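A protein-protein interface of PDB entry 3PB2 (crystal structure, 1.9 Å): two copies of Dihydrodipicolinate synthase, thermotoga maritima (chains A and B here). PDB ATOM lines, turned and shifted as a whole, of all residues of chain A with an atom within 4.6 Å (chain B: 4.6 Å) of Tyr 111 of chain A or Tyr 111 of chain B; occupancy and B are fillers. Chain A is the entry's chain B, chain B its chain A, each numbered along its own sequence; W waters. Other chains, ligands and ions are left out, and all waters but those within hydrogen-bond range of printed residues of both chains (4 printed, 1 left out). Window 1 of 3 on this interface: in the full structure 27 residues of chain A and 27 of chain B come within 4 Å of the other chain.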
ATOM      1  N   GLY A  83      19.134 -22.505 -19.107  1.00  0.00           N
ATOM      2  CA  GLY A  83      18.449 -21.419 -19.778  1.00  0.00           C
ATOM      3  C   GLY A  83      19.231 -20.930 -20.978  1.00  0.00           C
ATOM      4  O   GLY A  83      20.464 -20.904 -20.951  1.00  0.00           O
ATOM      5  N   THR A  84      18.519 -20.567 -22.039  1.00  0.00           N
ATOM      6  CA  THR A  84      19.147 -19.908 -23.180  1.00  0.00           C
ATOM      7  C   THR A  84      18.353 -18.651 -23.477  1.00  0.00           C
ATOM      8  O   THR A  84      17.463 -18.277 -22.702  1.00  0.00           O
ATOM      9  CB  THR A  84      19.216 -20.809 -24.427  1.00  0.00           C
ATOM     10  OG1 THR A  84      17.917 -20.923 -25.025  1.00  0.00           O
ATOM     11  CG2 THR A  84      19.761 -22.202 -24.053  1.00  0.00           C
ATOM     12  N   ASN A  85      18.677 -17.985 -24.579  1.00  0.00           N
ATOM     13  CA  ASN A  85      17.936 -16.787 -24.942  1.00  0.00           C
ATOM     14  C   ASN A  85      16.769 -17.083 -25.901  1.00  0.00           C
ATOM     15  O   ASN A  85      16.145 -16.164 -26.435  1.00  0.00           O
ATOM     16  CB  ASN A  85      18.877 -15.691 -25.467  1.00  0.00           C
ATOM     17  CG  ASN A  85      19.623 -16.100 -26.745  1.00  0.00           C
ATOM     18  OD1 ASN A  85      19.490 -17.225 -27.229  1.00  0.00           O
ATOM     19  ND2 ASN A  85      20.415 -15.180 -27.285  1.00  0.00           N
ATOM     20  N   VAL A 108      18.656 -18.479 -16.569  1.00  0.00           N
ATOM     21  CA  VAL A 108      19.119 -17.103 -16.763  1.00  0.00           C
ATOM     22  C   VAL A 108      18.114 -16.318 -17.594  1.00  0.00           C
ATOM     23  O   VAL A 108      17.430 -16.884 -18.446  1.00  0.00           O
ATOM     24  CB  VAL A 108      20.551 -17.042 -17.390  1.00  0.00           C
ATOM     25  CG1 VAL A 108      20.546 -17.514 -18.857  1.00  0.00           C
ATOM     26  CG2 VAL A 108      21.153 -15.627 -17.265  1.00  0.00           C
ATOM     27  N   THR A 109      17.969 -15.027 -17.312  1.00  0.00           N
ATOM     28  CA  THR A 109      17.181 -14.179 -18.203  1.00  0.00           C
ATOM     29  C   THR A 109      17.843 -14.272 -19.581  1.00  0.00           C
ATOM     30  O   THR A 109      19.065 -14.203 -19.679  1.00  0.00           O
ATOM     31  CB  THR A 109      17.242 -12.714 -17.781  1.00  0.00           C
ATOM     32  OG1 THR A 109      18.617 -12.307 -17.753  1.00  0.00           O
ATOM     33  CG2 THR A 109      16.616 -12.507 -16.385  1.00  0.00           C
ATOM     34  N   PRO A 110      17.047 -14.434 -20.648  1.00  0.00           N
ATOM     35  CA  PRO A 110      17.654 -14.429 -21.990  1.00  0.00           C
ATOM     36  C   PRO A 110      18.688 -13.327 -22.190  1.00  0.00           C
ATOM     37  O   PRO A 110      18.427 -12.139 -21.970  1.00  0.00           O
ATOM     38  CB  PRO A 110      16.455 -14.224 -22.902  1.00  0.00           C
ATOM     39  CG  PRO A 110      15.350 -15.016 -22.168  1.00  0.00           C
ATOM     40  CD  PRO A 110      15.607 -14.757 -20.690  1.00  0.00           C
ATOM     41  N   TYR A 111      19.869 -13.739 -22.634  1.00  0.00           N
ATOM     42  CA  TYR A 111      20.979 -12.815 -22.846  1.00  0.00           C
ATOM     43  C   TYR A 111      20.988 -12.360 -24.296  1.00  0.00           C
ATOM     44  O   TYR A 111      20.426 -13.037 -25.173  1.00  0.00           O
ATOM     45  CB  TYR A 111      22.306 -13.531 -22.542  1.00  0.00           C
ATOM     46  CG  TYR A 111      22.269 -14.985 -22.963  1.00  0.00           C
ATOM     47  CD1 TYR A 111      22.493 -15.348 -24.282  1.00  0.00           C
ATOM     48  CD2 TYR A 111      21.987 -15.992 -22.043  1.00  0.00           C
ATOM     49  CE1 TYR A 111      22.446 -16.689 -24.675  1.00  0.00           C
ATOM     50  CE2 TYR A 111      21.945 -17.314 -22.422  1.00  0.00           C
ATOM     51  CZ  TYR A 111      22.177 -17.654 -23.743  1.00  0.00           C
ATOM     52  OH  TYR A 111      22.138 -18.965 -24.132  1.00  0.00           O
ATOM     53  N   TYR A 112      21.609 -11.207 -24.539  1.00  0.00           N
ATOM     54  CA  TYR A 112      21.942 -10.759 -25.888  1.00  0.00           C
ATOM     55  C   TYR A 112      20.761 -10.201 -26.715  1.00  0.00           C
ATOM     56  O   TYR A 112      20.946  -9.189 -27.394  1.00  0.00           O
ATOM     57  CB  TYR A 112      22.688 -11.860 -26.634  1.00  0.00           C
ATOM     58  CG  TYR A 112      23.045 -11.529 -28.086  1.00  0.00           C
ATOM     59  CD1 TYR A 112      23.968 -10.533 -28.391  1.00  0.00           C
ATOM     60  CD2 TYR A 112      22.465 -12.225 -29.137  1.00  0.00           C
ATOM     61  CE1 TYR A 112      24.303 -10.237 -29.710  1.00  0.00           C
ATOM     62  CE2 TYR A 112      22.797 -11.945 -30.468  1.00  0.00           C
ATOM     63  CZ  TYR A 112      23.717 -10.947 -30.741  1.00  0.00           C
ATOM     64  OH  TYR A 112      24.050 -10.660 -32.048  1.00  0.00           O
ATOM     65  N   ASN A 113      19.565 -10.806 -26.637  1.00  0.00           N
ATOM     66  CA  ASN A 113      18.394 -10.261 -27.366  1.00  0.00           C
ATOM     67  C   ASN A 113      17.525  -9.216 -26.631  1.00  0.00           C
ATOM     68  O   ASN A 113      16.541  -8.698 -27.195  1.00  0.00           O
ATOM     69  CB  ASN A 113      17.518 -11.362 -28.021  1.00  0.00           C
ATOM     70  CG  ASN A 113      17.073 -12.456 -27.043  1.00  0.00           C
ATOM     71  OD1 ASN A 113      17.325 -12.389 -25.835  1.00  0.00           O
ATOM     72  ND2 ASN A 113      16.388 -13.475 -27.576  1.00  0.00           N
ATOM     73  N   THR A 144      24.143 -10.207 -19.404  1.00  0.00           N
ATOM     74  CA  THR A 144      23.034 -10.482 -20.336  1.00  0.00           C
ATOM     75  C   THR A 144      22.582  -9.276 -21.157  1.00  0.00           C
ATOM     76  O   THR A 144      21.954  -9.433 -22.211  1.00  0.00           O
ATOM     77  CB  THR A 144      21.803 -10.945 -19.551  1.00  0.00           C
ATOM     78  OG1 THR A 144      21.384  -9.873 -18.707  1.00  0.00           O
ATOM     79  CG2 THR A 144      22.148 -12.201 -18.687  1.00  0.00           C
ATOM     80  N   GLY B  83      27.390 -16.560 -35.182  1.00  0.00           N
ATOM     81  CA  GLY B  83      28.266 -16.544 -34.025  1.00  0.00           C
ATOM     82  C   GLY B  83      27.499 -16.840 -32.761  1.00  0.00           C
ATOM     83  O   GLY B  83      26.409 -16.301 -32.575  1.00  0.00           O
ATOM     84  N   THR B  84      28.043 -17.717 -31.914  1.00  0.00           N
ATOM     85  CA  THR B  84      27.520 -17.894 -30.573  1.00  0.00           C
ATOM     86  C   THR B  84      28.644 -17.607 -29.579  1.00  0.00           C
ATOM     87  O   THR B  84      29.697 -17.080 -29.960  1.00  0.00           O
ATOM     88  CB  THR B  84      26.971 -19.335 -30.330  1.00  0.00           C
ATOM     89  OG1 THR B  84      28.068 -20.259 -30.233  1.00  0.00           O
ATOM     90  CG2 THR B  84      26.018 -19.766 -31.464  1.00  0.00           C
ATOM     91  N   ASN B  85      28.429 -17.954 -28.314  1.00  0.00           N
ATOM     92  CA  ASN B  85      29.466 -17.745 -27.304  1.00  0.00           C
ATOM     93  C   ASN B  85      30.341 -18.988 -27.083  1.00  0.00           C
ATOM     94  O   ASN B  85      31.181 -19.014 -26.177  1.00  0.00           O
ATOM     95  CB  ASN B  85      28.875 -17.201 -25.983  1.00  0.00           C
ATOM     96  CG  ASN B  85      27.798 -18.105 -25.403  1.00  0.00           C
ATOM     97  OD1 ASN B  85      27.483 -19.146 -25.971  1.00  0.00           O
ATOM     98  ND2 ASN B  85      27.249 -17.724 -24.248  1.00  0.00           N
ATOM     99  N   VAL B 108      29.486 -12.336 -34.080  1.00  0.00           N
ATOM    100  CA  VAL B 108      29.457 -11.483 -32.878  1.00  0.00           C
ATOM    101  C   VAL B 108      30.535 -11.922 -31.882  1.00  0.00           C
ATOM    102  O   VAL B 108      30.881 -13.110 -31.807  1.00  0.00           O
ATOM    103  CB  VAL B 108      28.050 -11.509 -32.201  1.00  0.00           C
ATOM    104  CG1 VAL B 108      27.775 -12.875 -31.563  1.00  0.00           C
ATOM    105  CG2 VAL B 108      27.894 -10.365 -31.138  1.00  0.00           C
ATOM    106  N   THR B 109      31.084 -10.976 -31.135  1.00  0.00           N
ATOM    107  CA  THR B 109      31.937 -11.335 -29.996  1.00  0.00           C
ATOM    108  C   THR B 109      31.065 -12.189 -29.076  1.00  0.00           C
ATOM    109  O   THR B 109      29.919 -11.834 -28.797  1.00  0.00           O
ATOM    110  CB  THR B 109      32.332 -10.109 -29.180  1.00  0.00           C
ATOM    111  OG1 THR B 109      31.130  -9.440 -28.781  1.00  0.00           O
ATOM    112  CG2 THR B 109      33.187  -9.138 -29.998  1.00  0.00           C
ATOM    113  N   PRO B 110      31.600 -13.314 -28.595  1.00  0.00           N
ATOM    114  CA  PRO B 110      30.849 -14.143 -27.641  1.00  0.00           C
ATOM    115  C   PRO B 110      30.145 -13.318 -26.543  1.00  0.00           C
ATOM    116  O   PRO B 110      30.781 -12.513 -25.855  1.00  0.00           O
ATOM    117  CB  PRO B 110      31.941 -15.014 -27.039  1.00  0.00           C
ATOM    118  CG  PRO B 110      32.818 -15.313 -28.250  1.00  0.00           C
ATOM    119  CD  PRO B 110      32.856 -13.963 -29.018  1.00  0.00           C
ATOM    120  N   TYR B 111      28.844 -13.525 -26.399  1.00  0.00           N
ATOM    121  CA  TYR B 111      28.046 -12.814 -25.397  1.00  0.00           C
ATOM    122  C   TYR B 111      27.963 -13.621 -24.115  1.00  0.00           C
ATOM    123  O   TYR B 111      28.180 -14.833 -24.117  1.00  0.00           O
ATOM    124  CB  TYR B 111      26.626 -12.599 -25.942  1.00  0.00           C
ATOM    125  CG  TYR B 111      26.135 -13.821 -26.675  1.00  0.00           C
ATOM    126  CD1 TYR B 111      25.677 -14.940 -25.984  1.00  0.00           C
ATOM    127  CD2 TYR B 111      26.180 -13.876 -28.062  1.00  0.00           C
ATOM    128  CE1 TYR B 111      25.240 -16.085 -26.670  1.00  0.00           C
ATOM    129  CE2 TYR B 111      25.752 -14.996 -28.749  1.00  0.00           C
ATOM    130  CZ  TYR B 111      25.293 -16.094 -28.064  1.00  0.00           C
ATOM    131  OH  TYR B 111      24.886 -17.187 -28.797  1.00  0.00           O
ATOM    132  N   TYR B 112      27.678 -12.924 -23.016  1.00  0.00           N
ATOM    133  CA  TYR B 112      27.343 -13.559 -21.745  1.00  0.00           C
ATOM    134  C   TYR B 112      28.559 -14.112 -20.989  1.00  0.00           C
ATOM    135  O   TYR B 112      28.696 -13.868 -19.793  1.00  0.00           O
ATOM    136  CB  TYR B 112      26.270 -14.628 -21.962  1.00  0.00           C
ATOM    137  CG  TYR B 112      25.834 -15.330 -20.705  1.00  0.00           C
ATOM    138  CD1 TYR B 112      25.108 -14.654 -19.732  1.00  0.00           C
ATOM    139  CD2 TYR B 112      26.131 -16.665 -20.496  1.00  0.00           C
ATOM    140  CE1 TYR B 112      24.713 -15.282 -18.573  1.00  0.00           C
ATOM    141  CE2 TYR B 112      25.737 -17.313 -19.334  1.00  0.00           C
ATOM    142  CZ  TYR B 112      25.027 -16.612 -18.378  1.00  0.00           C
ATOM    143  OH  TYR B 112      24.620 -17.236 -17.223  1.00  0.00           O
ATOM    144  N   ASN B 113      29.455 -14.830 -21.669  1.00  0.00           N
ATOM    145  CA  ASN B 113      30.649 -15.337 -20.962  1.00  0.00           C
ATOM    146  C   ASN B 113      31.839 -14.370 -20.823  1.00  0.00           C
ATOM    147  O   ASN B 113      32.861 -14.713 -20.204  1.00  0.00           O
ATOM    148  CB  ASN B 113      31.092 -16.760 -21.419  1.00  0.00           C
ATOM    149  CG  ASN B 113      31.305 -16.892 -22.931  1.00  0.00           C
ATOM    150  OD1 ASN B 113      31.268 -15.924 -23.685  1.00  0.00           O
ATOM    151  ND2 ASN B 113      31.553 -18.128 -23.372  1.00  0.00           N
ATOM    152  N   ARG B 143      24.816  -5.430 -25.816  1.00  0.00           N
ATOM    153  CA  ARG B 143      24.075  -6.690 -25.875  1.00  0.00           C
ATOM    154  C   ARG B 143      24.895  -7.860 -25.337  1.00  0.00           C
ATOM    155  O   ARG B 143      24.343  -8.823 -24.797  1.00  0.00           O
ATOM    156  CB  ARG B 143      23.662  -7.018 -27.319  1.00  0.00           C
ATOM    157  CG  ARG B 143      22.525  -6.149 -27.867  1.00  0.00           C
ATOM    158  CD  ARG B 143      22.177  -6.591 -29.277  1.00  0.00           C
ATOM    159  NE  ARG B 143      21.083  -5.806 -29.852  1.00  0.00           N
ATOM    160  CZ  ARG B 143      19.804  -6.188 -29.802  1.00  0.00           C
ATOM    161  NH1 ARG B 143      18.854  -5.431 -30.345  1.00  0.00           N
ATOM    162  NH2 ARG B 143      19.477  -7.326 -29.191  1.00  0.00           N
ATOM    163  N   THR B 144      26.218  -7.778 -25.482  1.00  0.00           N
ATOM    164  CA  THR B 144      27.060  -8.949 -25.212  1.00  0.00           C
ATOM    165  C   THR B 144      27.759  -8.920 -23.851  1.00  0.00           C
ATOM    166  O   THR B 144      28.188  -9.963 -23.351  1.00  0.00           O
ATOM    167  CB  THR B 144      28.162  -9.069 -26.269  1.00  0.00           C
ATOM    168  OG1 THR B 144      29.024  -7.937 -26.136  1.00  0.00           O
ATOM    169  CG2 THR B 144      27.562  -9.084 -27.691  1.00  0.00           C
HETATM  170  O   HOH W   1      23.302 -19.360 -27.194  1.00  0.00           O
HETATM  171  O   HOH W   2      22.070 -16.101 -29.570  1.00  0.00           O
HETATM  172  O   HOH W   3      24.785 -11.227 -23.397  1.00  0.00           O
HETATM  173  O   HOH W   4      16.743  -8.481 -29.947  1.00  0.00           O
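NH2 of Arg 143 of chain B lies within hydrogen-bond range of O of Tyr 112 of chain A.
OD1 of Asn 113 of chain A lies close to O of Tyr 111 of chain A, 3.2 Å away.
The backbone carbonyl oxygen (O) of Thr 144 of chain B lies within hydrogen-bond range of the backbone NH (N) of Tyr 112 of chain B (3.0 Å).
O of Tyr 111 of chain B sits close to OD1 of Asn 113 of chain B (3.3 Å).
The side-chain amide nitrogen (ND2) of Asn 85 of chain B is in hydrogen-bond range of the backbone carbonyl oxygen (O) of Tyr 111 of chain B, 3.0 Å away.
The side-chain amide nitrogen (ND2) of Asn 113 of chain A sits at hydrogen-bond distance from the backbone carbonyl oxygen (O) of Asn 85 of chain A (2.9 Å).
The side-chain amide nitrogen (ND2) of Asn 85 of chain A is in hydrogen-bond range of the backbone carbonyl oxygen (O) of Tyr 111 of chain A (3.0 Å).
Among the printed residues, merely in contact across the chains: Val 108 of chain A with Tyr 112 of chain B, Tyr 111 of chain A with Tyr 111 of chain B, Tyr 112 of chain A with Val 108 of chain B, Tyr 112 of chain A with Tyr 111 of chain B, Tyr 112 of chain A with Thr 144 of chain B, Asn 113 of chain A with Arg 143 of chain B, Thr 144 of chain A with Tyr 112 of chain B and Thr 144 of chain A with Arg 143 of chain B.
Of the printed residues of chain B, Val 108 of chain A touches Tyr 112.
Of the printed residues of chain B, Tyr 111 of chain A touches Tyr 111.
Of the printed residues of chain A, Val 108 of chain B touches Tyr 112.
Tyr 111 of chain B touches two residues of chain A.
The nearest residue of chain B that does not touch Tyr 111 of chain A is Tyr 112 of chain B (4.1 Å).
The nearest printed residue of chain A that does not touch Tyr 111 of chain B is Asn 85 of chain A (4.9 Å).
Hydrophobic or aromatic side chains of chain B that line the printed part of chain A: Val 108, Tyr 111 and Tyr 112.
Val 108 of chain A touches Tyr 112 of chain B, and with the chains exchanged Tyr 112 of chain A touches Val 108 of chain B.
Tyr 111 of chain A touches its own counterpart, Tyr 111 of chain B.
Tyr 112 of chain A touches Tyr 111 of chain B, but with the chains exchanged Tyr 111 of chain A does not touch Tyr 112 of chain B (4.1 Å).
Tyr 112 of chain A touches Thr 144 of chain B, and with the chains exchanged Thr 144 of chain A touches Tyr 112 of chain B.
Of the 9 pairs that touch across the chains among the printed residues, 5 have their exchanged pair printed and touching as well.
Water W4 lies within hydrogen-bond range of the backbone carbonyl oxygen (O) of Asn 113 of chain A (2.8 Å) and the guanidinium group (NH2) of Arg 143 of chain B (3.1 Å).
Water W3 lies within hydrogen-bond range of the backbone carbonyl oxygen (O) of Arg 143 of chain B, the backbone NH (N) of Tyr 112 of chain A and the backbone NH (N) of Tyr 112 of chain B.
Water W2 lies within hydrogen-bond range of the side-chain amide nitrogen (ND2) of Asn 85 of chain A and the side-chain hydroxyl (OH) of Tyr 111 of chain B.
Water W1 lies within hydrogen-bond range of OH of Tyr 111 of chain B (3.1 Å) and OH of Tyr 111 of chain A (3.3 Å).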
